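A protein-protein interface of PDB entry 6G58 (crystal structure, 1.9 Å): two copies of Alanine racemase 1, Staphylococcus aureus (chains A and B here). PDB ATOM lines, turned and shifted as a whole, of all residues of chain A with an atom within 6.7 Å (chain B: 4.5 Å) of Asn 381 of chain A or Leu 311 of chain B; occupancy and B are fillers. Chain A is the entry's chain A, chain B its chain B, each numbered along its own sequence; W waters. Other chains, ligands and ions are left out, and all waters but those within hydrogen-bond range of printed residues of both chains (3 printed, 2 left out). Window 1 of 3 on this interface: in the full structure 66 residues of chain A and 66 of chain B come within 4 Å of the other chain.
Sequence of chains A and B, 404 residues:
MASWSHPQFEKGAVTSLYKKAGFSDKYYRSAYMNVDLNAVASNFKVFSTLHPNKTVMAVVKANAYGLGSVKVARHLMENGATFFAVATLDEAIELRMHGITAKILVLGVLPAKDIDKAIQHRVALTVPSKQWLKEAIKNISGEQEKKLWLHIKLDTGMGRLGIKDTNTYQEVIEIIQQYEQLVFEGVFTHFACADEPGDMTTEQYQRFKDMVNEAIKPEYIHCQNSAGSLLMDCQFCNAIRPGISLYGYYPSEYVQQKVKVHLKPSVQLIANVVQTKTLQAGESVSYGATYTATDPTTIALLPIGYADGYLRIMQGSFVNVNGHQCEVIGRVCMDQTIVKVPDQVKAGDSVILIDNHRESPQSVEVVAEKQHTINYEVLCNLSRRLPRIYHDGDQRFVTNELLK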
ATOM      1  N   TYR A  65     -18.020  22.400  21.057  1.00  0.00           N
ATOM      2  CA  TYR A  65     -18.859  21.385  20.421  1.00  0.00           C
ATOM      3  C   TYR A  65     -18.627  20.020  21.122  1.00  0.00           C
ATOM      4  O   TYR A  65     -18.661  18.966  20.500  1.00  0.00           O
ATOM      5  CB  TYR A  65     -18.615  21.303  18.911  1.00  0.00           C
ATOM      6  CG  TYR A  65     -19.014  22.501  18.042  1.00  0.00           C
ATOM      7  CD1 TYR A  65     -18.779  23.795  18.449  1.00  0.00           C
ATOM      8  CD2 TYR A  65     -19.533  22.325  16.778  1.00  0.00           C
ATOM      9  CE1 TYR A  65     -19.104  24.877  17.650  1.00  0.00           C
ATOM     10  CE2 TYR A  65     -19.880  23.410  15.972  1.00  0.00           C
ATOM     11  CZ  TYR A  65     -19.652  24.689  16.414  1.00  0.00           C
ATOM     12  OH  TYR A  65     -19.922  25.841  15.706  1.00  0.00           O
ATOM     13  N   TYR A 306     -27.165   5.970  27.400  1.00  0.00           N
ATOM     14  CA  TYR A 306     -27.747   7.228  26.939  1.00  0.00           C
ATOM     15  C   TYR A 306     -27.518   8.434  27.829  1.00  0.00           C
ATOM     16  O   TYR A 306     -27.554   9.566  27.320  1.00  0.00           O
ATOM     17  CB  TYR A 306     -29.217   7.094  26.548  1.00  0.00           C
ATOM     18  CG  TYR A 306     -30.196   6.737  27.631  1.00  0.00           C
ATOM     19  CD1 TYR A 306     -30.658   7.694  28.529  1.00  0.00           C
ATOM     20  CD2 TYR A 306     -30.700   5.453  27.709  1.00  0.00           C
ATOM     21  CE1 TYR A 306     -31.609   7.370  29.499  1.00  0.00           C
ATOM     22  CE2 TYR A 306     -31.677   5.103  28.657  1.00  0.00           C
ATOM     23  CZ  TYR A 306     -32.124   6.058  29.545  1.00  0.00           C
ATOM     24  OH  TYR A 306     -33.051   5.754  30.518  1.00  0.00           O
ATOM     25  N   ALA A 307     -27.196   8.241  29.105  1.00  0.00           N
ATOM     26  CA  ALA A 307     -26.776   9.364  29.928  1.00  0.00           C
ATOM     27  C   ALA A 307     -25.411   9.892  29.543  1.00  0.00           C
ATOM     28  O   ALA A 307     -25.050  11.000  29.950  1.00  0.00           O
ATOM     29  CB  ALA A 307     -26.826   9.050  31.420  1.00  0.00           C
ATOM     30  N   ASP A 308     -24.649   9.109  28.780  1.00  0.00           N
ATOM     31  CA  ASP A 308     -23.387   9.569  28.196  1.00  0.00           C
ATOM     32  C   ASP A 308     -23.547  10.245  26.840  1.00  0.00           C
ATOM     33  O   ASP A 308     -22.558  10.817  26.327  1.00  0.00           O
ATOM     34  CB  ASP A 308     -22.414   8.394  28.094  1.00  0.00           C
ATOM     35  CG  ASP A 308     -22.177   7.757  29.448  1.00  0.00           C
ATOM     36  OD1 ASP A 308     -21.600   8.480  30.320  1.00  0.00           O
ATOM     37  OD2 ASP A 308     -22.618   6.595  29.674  1.00  0.00           O
ATOM     38  N   GLY A 309     -24.757  10.199  26.278  1.00  0.00           N
ATOM     39  CA  GLY A 309     -25.009  10.748  24.949  1.00  0.00           C
ATOM     40  C   GLY A 309     -25.093   9.733  23.837  1.00  0.00           C
ATOM     41  O   GLY A 309     -25.315  10.123  22.671  1.00  0.00           O
ATOM     42  N   TYR A 310     -24.923   8.445  24.166  1.00  0.00           N
ATOM     43  CA  TYR A 310     -25.122   7.351  23.206  1.00  0.00           C
ATOM     44  C   TYR A 310     -26.612   6.969  23.286  1.00  0.00           C
ATOM     45  O   TYR A 310     -27.030   6.076  24.050  1.00  0.00           O
ATOM     46  CB  TYR A 310     -24.162   6.185  23.485  1.00  0.00           C
ATOM     47  CG  TYR A 310     -23.994   5.276  22.279  1.00  0.00           C
ATOM     48  CD1 TYR A 310     -23.262   5.693  21.167  1.00  0.00           C
ATOM     49  CD2 TYR A 310     -24.572   4.012  22.253  1.00  0.00           C
ATOM     50  CE1 TYR A 310     -23.133   4.892  20.035  1.00  0.00           C
ATOM     51  CE2 TYR A 310     -24.455   3.188  21.139  1.00  0.00           C
ATOM     52  CZ  TYR A 310     -23.755   3.628  20.017  1.00  0.00           C
ATOM     53  OH  TYR A 310     -23.629   2.795  18.941  1.00  0.00           O
ATOM     54  N   LEU A 311     -27.419   7.714  22.557  1.00  0.00           N
ATOM     55  CA  LEU A 311     -28.878   7.726  22.789  1.00  0.00           C
ATOM     56  C   LEU A 311     -29.578   6.402  22.479  1.00  0.00           C
ATOM     57  O   LEU A 311     -29.043   5.533  21.759  1.00  0.00           O
ATOM     58  CB  LEU A 311     -29.510   8.860  21.978  1.00  0.00           C
ATOM     59  CG  LEU A 311     -29.001  10.298  22.262  1.00  0.00           C
ATOM     60  CD1 LEU A 311     -29.910  11.290  21.542  1.00  0.00           C
ATOM     61  CD2 LEU A 311     -28.933  10.643  23.757  1.00  0.00           C
ATOM     62  N   GLN A 371     -29.330   8.720  14.396  1.00  0.00           N
ATOM     63  CA  GLN A 371     -30.048   9.640  15.268  1.00  0.00           C
ATOM     64  C   GLN A 371     -31.034  10.573  14.578  1.00  0.00           C
ATOM     65  O   GLN A 371     -31.722  11.347  15.270  1.00  0.00           O
ATOM     66  CB  GLN A 371     -29.038  10.468  16.107  1.00  0.00           C
ATOM     67  CG  GLN A 371     -28.229   9.651  17.109  1.00  0.00           C
ATOM     68  CD  GLN A 371     -27.315  10.489  17.977  1.00  0.00           C
ATOM     69  OE1 GLN A 371     -27.545  11.701  18.161  1.00  0.00           O
ATOM     70  NE2 GLN A 371     -26.317   9.824  18.598  1.00  0.00           N
ATOM     71  N   THR A 373     -30.395  13.183  12.767  1.00  0.00           N
ATOM     72  CA  THR A 373     -29.960  14.526  13.115  1.00  0.00           C
ATOM     73  C   THR A 373     -28.700  14.888  12.317  1.00  0.00           C
ATOM     74  O   THR A 373     -28.382  14.229  11.345  1.00  0.00           O
ATOM     75  CB  THR A 373     -29.767  14.694  14.656  1.00  0.00           C
ATOM     76  OG1 THR A 373     -29.688  16.089  14.994  1.00  0.00           O
ATOM     77  CG2 THR A 373     -28.567  13.959  15.150  1.00  0.00           C
ATOM     78  N   TYR A 376     -23.305  18.002  14.246  1.00  0.00           N
ATOM     79  CA  TYR A 376     -23.246  18.979  15.341  1.00  0.00           C
ATOM     80  C   TYR A 376     -23.896  18.451  16.633  1.00  0.00           C
ATOM     81  O   TYR A 376     -23.333  18.591  17.747  1.00  0.00           O
ATOM     82  CB  TYR A 376     -23.958  20.277  14.992  1.00  0.00           C
ATOM     83  CG  TYR A 376     -23.442  21.087  13.794  1.00  0.00           C
ATOM     84  CD1 TYR A 376     -23.796  20.756  12.478  1.00  0.00           C
ATOM     85  CD2 TYR A 376     -22.689  22.229  13.995  1.00  0.00           C
ATOM     86  CE1 TYR A 376     -23.340  21.519  11.404  1.00  0.00           C
ATOM     87  CE2 TYR A 376     -22.257  23.009  12.928  1.00  0.00           C
ATOM     88  CZ  TYR A 376     -22.587  22.637  11.625  1.00  0.00           C
ATOM     89  OH  TYR A 376     -22.144  23.450  10.593  1.00  0.00           O
ATOM     90  N   GLU A 377     -25.091  17.871  16.489  1.00  0.00           N
ATOM     91  CA  GLU A 377     -25.850  17.434  17.649  1.00  0.00           C
ATOM     92  C   GLU A 377     -25.288  16.167  18.244  1.00  0.00           C
ATOM     93  O   GLU A 377     -25.311  15.987  19.469  1.00  0.00           O
ATOM     94  CB  GLU A 377     -27.334  17.292  17.298  1.00  0.00           C
ATOM     95  CG  GLU A 377     -28.210  16.987  18.528  1.00  0.00           C
ATOM     96  CD  GLU A 377     -29.679  17.012  18.208  1.00  0.00           C
ATOM     97  OE1 GLU A 377     -30.190  16.013  17.666  1.00  0.00           O
ATOM     98  OE2 GLU A 377     -30.322  18.021  18.537  1.00  0.00           O
ATOM     99  N   VAL A 378     -24.731  15.296  17.407  1.00  0.00           N
ATOM    100  CA  VAL A 378     -24.119  14.068  17.918  1.00  0.00           C
ATOM    101  C   VAL A 378     -22.998  14.436  18.927  1.00  0.00           C
ATOM    102  O   VAL A 378     -22.901  13.837  20.009  1.00  0.00           O
ATOM    103  CB  VAL A 378     -23.534  13.190  16.800  1.00  0.00           C
ATOM    104  CG1 VAL A 378     -22.739  12.019  17.375  1.00  0.00           C
ATOM    105  CG2 VAL A 378     -24.655  12.656  15.901  1.00  0.00           C
ATOM    106  N   LEU A 379     -22.177  15.401  18.542  1.00  0.00           N
ATOM    107  CA  LEU A 379     -21.069  15.882  19.373  1.00  0.00           C
ATOM    108  C   LEU A 379     -21.579  16.611  20.633  1.00  0.00           C
ATOM    109  O   LEU A 379     -21.071  16.374  21.721  1.00  0.00           O
ATOM    110  CB  LEU A 379     -20.144  16.803  18.581  1.00  0.00           C
ATOM    111  CG  LEU A 379     -19.457  16.166  17.357  1.00  0.00           C
ATOM    112  CD1 LEU A 379     -18.876  17.227  16.442  1.00  0.00           C
ATOM    113  CD2 LEU A 379     -18.380  15.181  17.792  1.00  0.00           C
ATOM    114  N   CYS A 380     -22.569  17.487  20.485  1.00  0.00           N
ATOM    115  CA  CYS A 380     -23.094  18.199  21.623  1.00  0.00           C
ATOM    116  C   CYS A 380     -23.761  17.274  22.655  1.00  0.00           C
ATOM    117  O   CYS A 380     -23.775  17.607  23.842  1.00  0.00           O
ATOM    118  CB  CYS A 380     -24.069  19.303  21.199  1.00  0.00           C
ATOM    119  SG  CYS A 380     -23.218  20.686  20.415  1.00  0.00           S
ATOM    120  N   ASN A 381     -24.303  16.149  22.196  1.00  0.00           N
ATOM    121  CA  ASN A 381     -24.962  15.188  23.082  1.00  0.00           C
ATOM    122  C   ASN A 381     -23.985  14.499  24.080  1.00  0.00           C
ATOM    123  O   ASN A 381     -24.426  13.943  25.048  1.00  0.00           O
ATOM    124  CB  ASN A 381     -25.598  14.045  22.270  1.00  0.00           C
ATOM    125  CG  ASN A 381     -26.904  14.398  21.627  1.00  0.00           C
ATOM    126  OD1 ASN A 381     -27.583  15.357  22.011  1.00  0.00           O
ATOM    127  ND2 ASN A 381     -27.291  13.584  20.624  1.00  0.00           N
ATOM    128  N   LEU A 382     -22.693  14.482  23.794  1.00  0.00           N
ATOM    129  CA  LEU A 382     -21.732  13.734  24.594  1.00  0.00           C
ATOM    130  C   LEU A 382     -21.613  14.395  25.955  1.00  0.00           C
ATOM    131  O   LEU A 382     -21.289  15.561  26.053  1.00  0.00           O
ATOM    132  CB  LEU A 382     -20.388  13.634  23.867  1.00  0.00           C
ATOM    133  CG  LEU A 382     -20.475  12.895  22.509  1.00  0.00           C
ATOM    134  CD1 LEU A 382     -19.122  12.951  21.833  1.00  0.00           C
ATOM    135  CD2 LEU A 382     -20.965  11.467  22.638  1.00  0.00           C
ATOM    136  N   SER A 383     -21.947  13.663  27.005  1.00  0.00           N
ATOM    137  CA  SER A 383     -22.294  14.306  28.268  1.00  0.00           C
ATOM    138  C   SER A 383     -21.071  14.536  29.141  1.00  0.00           C
ATOM    139  O   SER A 383     -19.975  14.056  28.859  1.00  0.00           O
ATOM    140  CB  SER A 383     -23.341  13.499  29.017  1.00  0.00           C
ATOM    141  OG  SER A 383     -22.744  12.517  29.844  1.00  0.00           O
ATOM    142  N   ARG A 384     -21.295  15.268  30.212  1.00  0.00           N
ATOM    143  CA  ARG A 384     -20.250  15.570  31.184  1.00  0.00           C
ATOM    144  C   ARG A 384     -19.642  14.313  31.863  1.00  0.00           C
ATOM    145  O   ARG A 384     -18.560  14.393  32.438  1.00  0.00           O
ATOM    146  CB  ARG A 384     -20.799  16.492  32.253  1.00  0.00           C
ATOM    147  CG  ARG A 384     -21.848  15.862  33.160  1.00  0.00           C
ATOM    148  CD  ARG A 384     -22.463  16.841  34.118  1.00  0.00           C
ATOM    149  NE  ARG A 384     -21.686  17.114  35.329  1.00  0.00           N
ATOM    150  CZ  ARG A 384     -21.600  16.313  36.392  1.00  0.00           C
ATOM    151  NH1 ARG A 384     -22.183  15.098  36.408  1.00  0.00           N
ATOM    152  NH2 ARG A 384     -20.891  16.722  37.445  1.00  0.00           N
ATOM    153  N   LEU A 386     -18.566  11.621  30.426  1.00  0.00           N
ATOM    154  CA  LEU A 386     -17.441  11.096  29.678  1.00  0.00           C
ATOM    155  C   LEU A 386     -16.165  11.882  29.940  1.00  0.00           C
ATOM    156  O   LEU A 386     -16.095  13.073  29.649  1.00  0.00           O
ATOM    157  CB  LEU A 386     -17.716  11.084  28.165  1.00  0.00           C
ATOM    158  CG  LEU A 386     -18.786  10.123  27.717  1.00  0.00           C
ATOM    159  CD1 LEU A 386     -19.207  10.537  26.309  1.00  0.00           C
ATOM    160  CD2 LEU A 386     -18.294   8.690  27.748  1.00  0.00           C
ATOM    161  N   ARG A 388     -12.677  13.394  28.863  1.00  0.00           N
ATOM    162  CA  ARG A 388     -12.000  13.762  27.630  1.00  0.00           C
ATOM    163  C   ARG A 388     -10.549  13.513  27.831  1.00  0.00           C
ATOM    164  O   ARG A 388      -9.961  14.048  28.764  1.00  0.00           O
ATOM    165  CB  ARG A 388     -12.208  15.221  27.281  1.00  0.00           C
ATOM    166  CG  ARG A 388     -13.478  15.525  26.505  1.00  0.00           C
ATOM    167  CD  ARG A 388     -14.725  15.400  27.338  1.00  0.00           C
ATOM    168  NE  ARG A 388     -15.882  15.919  26.653  1.00  0.00           N
ATOM    169  CZ  ARG A 388     -17.157  15.663  26.952  1.00  0.00           C
ATOM    170  NH1 ARG A 388     -17.491  14.894  27.988  1.00  0.00           N
ATOM    171  NH2 ARG A 388     -18.119  16.194  26.202  1.00  0.00           N
ATOM    172  N   TYR B 306     -30.045  23.177  21.077  1.00  0.00           N
ATOM    173  CA  TYR B 306     -29.740  21.758  21.220  1.00  0.00           C
ATOM    174  C   TYR B 306     -28.483  21.407  21.983  1.00  0.00           C
ATOM    175  O   TYR B 306     -28.420  20.305  22.538  1.00  0.00           O
ATOM    176  CB  TYR B 306     -29.839  20.997  19.906  1.00  0.00           C
ATOM    177  CG  TYR B 306     -28.856  21.341  18.822  1.00  0.00           C
ATOM    178  CD1 TYR B 306     -27.539  20.879  18.859  1.00  0.00           C
ATOM    179  CD2 TYR B 306     -29.263  22.118  17.745  1.00  0.00           C
ATOM    180  CE1 TYR B 306     -26.655  21.174  17.826  1.00  0.00           C
ATOM    181  CE2 TYR B 306     -28.407  22.409  16.700  1.00  0.00           C
ATOM    182  CZ  TYR B 306     -27.119  21.944  16.721  1.00  0.00           C
ATOM    183  OH  TYR B 306     -26.260  22.273  15.698  1.00  0.00           O
ATOM    184  N   GLY B 309     -29.578  20.549  25.336  1.00  0.00           N
ATOM    185  CA  GLY B 309     -30.436  19.363  25.434  1.00  0.00           C
ATOM    186  C   GLY B 309     -31.840  19.541  24.916  1.00  0.00           C
ATOM    187  O   GLY B 309     -32.619  18.596  24.999  1.00  0.00           O
ATOM    188  N   TYR B 310     -32.177  20.754  24.403  1.00  0.00           N
ATOM    189  CA  TYR B 310     -33.454  20.996  23.744  1.00  0.00           C
ATOM    190  C   TYR B 310     -33.258  20.642  22.271  1.00  0.00           C
ATOM    191  O   TYR B 310     -32.910  21.490  21.424  1.00  0.00           O
ATOM    192  CB  TYR B 310     -33.956  22.423  23.981  1.00  0.00           C
ATOM    193  CG  TYR B 310     -35.447  22.571  23.723  1.00  0.00           C
ATOM    194  CD1 TYR B 310     -36.387  22.025  24.606  1.00  0.00           C
ATOM    195  CD2 TYR B 310     -35.907  23.231  22.585  1.00  0.00           C
ATOM    196  CE1 TYR B 310     -37.752  22.127  24.358  1.00  0.00           C
ATOM    197  CE2 TYR B 310     -37.273  23.358  22.335  1.00  0.00           C
ATOM    198  CZ  TYR B 310     -38.197  22.799  23.213  1.00  0.00           C
ATOM    199  OH  TYR B 310     -39.539  22.938  22.943  1.00  0.00           O
ATOM    200  N   LEU B 311     -33.392  19.354  21.978  1.00  0.00           N
ATOM    201  CA  LEU B 311     -32.882  18.806  20.719  1.00  0.00           C
ATOM    202  C   LEU B 311     -33.607  19.315  19.457  1.00  0.00           C
ATOM    203  O   LEU B 311     -34.724  19.825  19.525  1.00  0.00           O
ATOM    204  CB  LEU B 311     -32.910  17.286  20.768  1.00  0.00           C
ATOM    205  CG  LEU B 311     -32.172  16.582  21.910  1.00  0.00           C
ATOM    206  CD1 LEU B 311     -32.176  15.097  21.635  1.00  0.00           C
ATOM    207  CD2 LEU B 311     -30.725  17.057  22.071  1.00  0.00           C
ATOM    208  N   ARG B 312     -32.961  19.116  18.305  1.00  0.00           N
ATOM    209  CA  ARG B 312     -33.479  19.611  17.026  1.00  0.00           C
ATOM    210  C   ARG B 312     -34.891  19.099  16.735  1.00  0.00           C
ATOM    211  O   ARG B 312     -35.710  19.807  16.167  1.00  0.00           O
ATOM    212  CB  ARG B 312     -32.544  19.263  15.875  1.00  0.00           C
ATOM    213  CG  ARG B 312     -31.269  20.072  15.960  1.00  0.00           C
ATOM    214  CD  ARG B 312     -30.236  19.724  14.933  1.00  0.00           C
ATOM    215  NE  ARG B 312     -30.583  20.111  13.561  1.00  0.00           N
ATOM    216  CZ  ARG B 312     -30.973  19.296  12.594  1.00  0.00           C
ATOM    217  NH1 ARG B 312     -31.201  18.013  12.812  1.00  0.00           N
ATOM    218  NH2 ARG B 312     -31.186  19.795  11.385  1.00  0.00           N
ATOM    219  N   ILE B 313     -35.164  17.865  17.155  1.00  0.00           N
ATOM    220  CA  ILE B 313     -36.471  17.262  16.921  1.00  0.00           C
ATOM    221  C   ILE B 313     -37.624  18.030  17.612  1.00  0.00           C
ATOM    222  O   ILE B 313     -38.780  17.804  17.309  1.00  0.00           O
ATOM    223  CB  ILE B 313     -36.455  15.774  17.330  1.00  0.00           C
ATOM    224  CG1 ILE B 313     -37.680  15.022  16.780  1.00  0.00           C
ATOM    225  CG2 ILE B 313     -36.311  15.632  18.841  1.00  0.00           C
ATOM    226  CD1 ILE B 313     -37.515  13.506  16.848  1.00  0.00           C
ATOM    227  N   MET B 314     -37.301  18.918  18.550  1.00  0.00           N
ATOM    228  CA  MET B 314     -38.305  19.753  19.206  1.00  0.00           C
ATOM    229  C   MET B 314     -38.993  20.757  18.277  1.00  0.00           C
ATOM    230  O   MET B 314     -40.045  21.287  18.622  1.00  0.00           O
ATOM    231  CB  MET B 314     -37.697  20.474  20.422  1.00  0.00           C
ATOM    232  CG  MET B 314     -37.183  19.553  21.539  1.00  0.00           C
ATOM    233  SD  MET B 314     -38.378  18.292  22.043  1.00  0.00           S
ATOM    234  CE  MET B 314     -39.626  19.293  22.833  1.00  0.00           C
ATOM    235  N   VAL B 332     -34.193  24.413  15.211  1.00  0.00           N
ATOM    236  CA  VAL B 332     -33.579  24.659  16.501  1.00  0.00           C
ATOM    237  C   VAL B 332     -32.068  24.717  16.266  1.00  0.00           C
ATOM    238  O   VAL B 332     -31.518  23.850  15.600  1.00  0.00           O
ATOM    239  CB  VAL B 332     -33.939  23.549  17.526  1.00  0.00           C
ATOM    240  CG1 VAL B 332     -33.272  23.816  18.869  1.00  0.00           C
ATOM    241  CG2 VAL B 332     -35.438  23.483  17.736  1.00  0.00           C
ATOM    242  N   GLN B 371     -39.654  13.678  21.142  1.00  0.00           N
ATOM    243  CA  GLN B 371     -38.311  13.121  20.949  1.00  0.00           C
ATOM    244  C   GLN B 371     -38.283  11.621  20.598  1.00  0.00           C
ATOM    245  O   GLN B 371     -37.192  11.079  20.341  1.00  0.00           O
ATOM    246  CB  GLN B 371     -37.440  13.368  22.202  1.00  0.00           C
ATOM    247  CG  GLN B 371     -37.133  14.823  22.482  1.00  0.00           C
ATOM    248  CD  GLN B 371     -36.154  15.053  23.630  1.00  0.00           C
ATOM    249  OE1 GLN B 371     -35.414  14.142  24.017  1.00  0.00           O
ATOM    250  NE2 GLN B 371     -36.110  16.293  24.145  1.00  0.00           N
ATOM    251  N   ASN B 381     -30.589  14.312  28.842  1.00  0.00           N
ATOM    252  CA  ASN B 381     -30.117  15.175  27.769  1.00  0.00           C
ATOM    253  C   ASN B 381     -29.758  16.611  28.222  1.00  0.00           C
ATOM    254  O   ASN B 381     -29.024  17.295  27.516  1.00  0.00           O
ATOM    255  CB  ASN B 381     -31.184  15.339  26.686  1.00  0.00           C
ATOM    256  CG  ASN B 381     -31.306  14.165  25.755  1.00  0.00           C
ATOM    257  OD1 ASN B 381     -30.400  13.335  25.630  1.00  0.00           O
ATOM    258  ND2 ASN B 381     -32.484  14.087  25.062  1.00  0.00           N
HETATM  259  O   HOH W   1     -28.192  14.880  24.753  1.00  0.00           O
HETATM  260  O   HOH W   2     -32.995  16.033  14.536  1.00  0.00           O
HETATM  261  O   HOH W   3     -32.897  15.891  17.308  1.00  0.00           O
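OG1 of Thr 373 of chain A sits at hydrogen-bond distance from NH1 of Arg 312 of chain B, at 3.3 Å.
The side-chain carboxylate (OE2) of Glu 377 of chain A sits at hydrogen-bond distance from the backbone NH (N) of Arg 312 of chain B (2.9 Å).
OE1 of Gln 371 of chain A lies within hydrogen-bond range of ND2 of Asn 381 of chain A.
The side-chain hydroxyl of Thr 373 of chain A sits at hydrogen-bond distance from the side-chain carboxylate of Glu 377 of chain A.
The side-chain sulfur (SG) of Cys 380 of chain A is in hydrogen-bond range of the backbone carbonyl oxygen (O) of Tyr 376 of chain A, at 3.4 Å.
The backbone carbonyl oxygen of Glu 377 of chain A lies close to the side-chain amide nitrogen of Asn 381 of chain A (3.3 Å).
The side-chain amide oxygen (OE1) of Gln 371 of chain B lies within hydrogen-bond range of the side-chain amide nitrogen (ND2) of Asn 381 of chain B.
Among the printed residues, pairs that only touch across the chains: Tyr 376 of chain A with Tyr 306 of chain B, Glu 377 of chain A with Tyr 306 of chain B, Glu 377 of chain A with Leu 311 of chain B, Asn 381 of chain A with Leu 311 of chain B and Leu 311 of chain A with Asn 381 of chain B.
Of the printed residues of chain B, Glu 377 of chain A touches Tyr 306 (3.3 Å), Leu 311 (3.5 Å) and Arg 312 (2.9 Å).
Asn 381 of chain A touches one residue of chain B.
Of the printed residues of chain A, Tyr 306 of chain B touches Tyr 376 and Glu 377.
Leu 311 of chain B touches just these residues of chain A: Glu 377 and Asn 381.
The nearest printed residue of chain B that does not touch Glu 377 of chain A is Ile 313 of chain B (5.0 Å).
Of the 10 printed residues of chain B, 4 touch a printed residue of chain A.
Printed residues of chain B that touch a printed residue of chain A: Tyr 306, Leu 311, Arg 312 and Asn 381.
Printed residues of chain A that touch a printed residue of chain B: Leu 311, Thr 373, Tyr 376, Glu 377 and Asn 381.
Hydrophobic or aromatic side chains of chain A within 4 Å of the printed part of chain B: Leu 311 and Tyr 376.
Leu 311 of chain A touches Asn 381 of chain B, and with the chains exchanged Asn 381 of chain A touches Leu 311 of chain B.
Positions printed for both chains: 306, 309, 310, 311, 371 and 381.
Of the 7 pairs that touch across the chains among the printed residues, 2 have their exchanged pair printed and touching as well.
Water W3 lies within hydrogen-bond range of the side-chain carboxylate (OE1) of Glu 377 of chain A (2.7 Å), the backbone NH (N) of Ile 313 of chain B (3.0 Å) and the backbone NH (N) of Arg 312 of chain B (3.4 Å).
Water W1 lies within hydrogen-bond range of the side-chain amide oxygen (OD1) of Asn 381 of chain B (2.8 Å) and the side-chain amide oxygen (OD1) of Asn 381 of chain A (2.8 Å).
Water W2 bridges NH1 of Arg 312 of chain B (3.2 Å) and OG1 of Thr 373 of chain A (3.3 Å).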
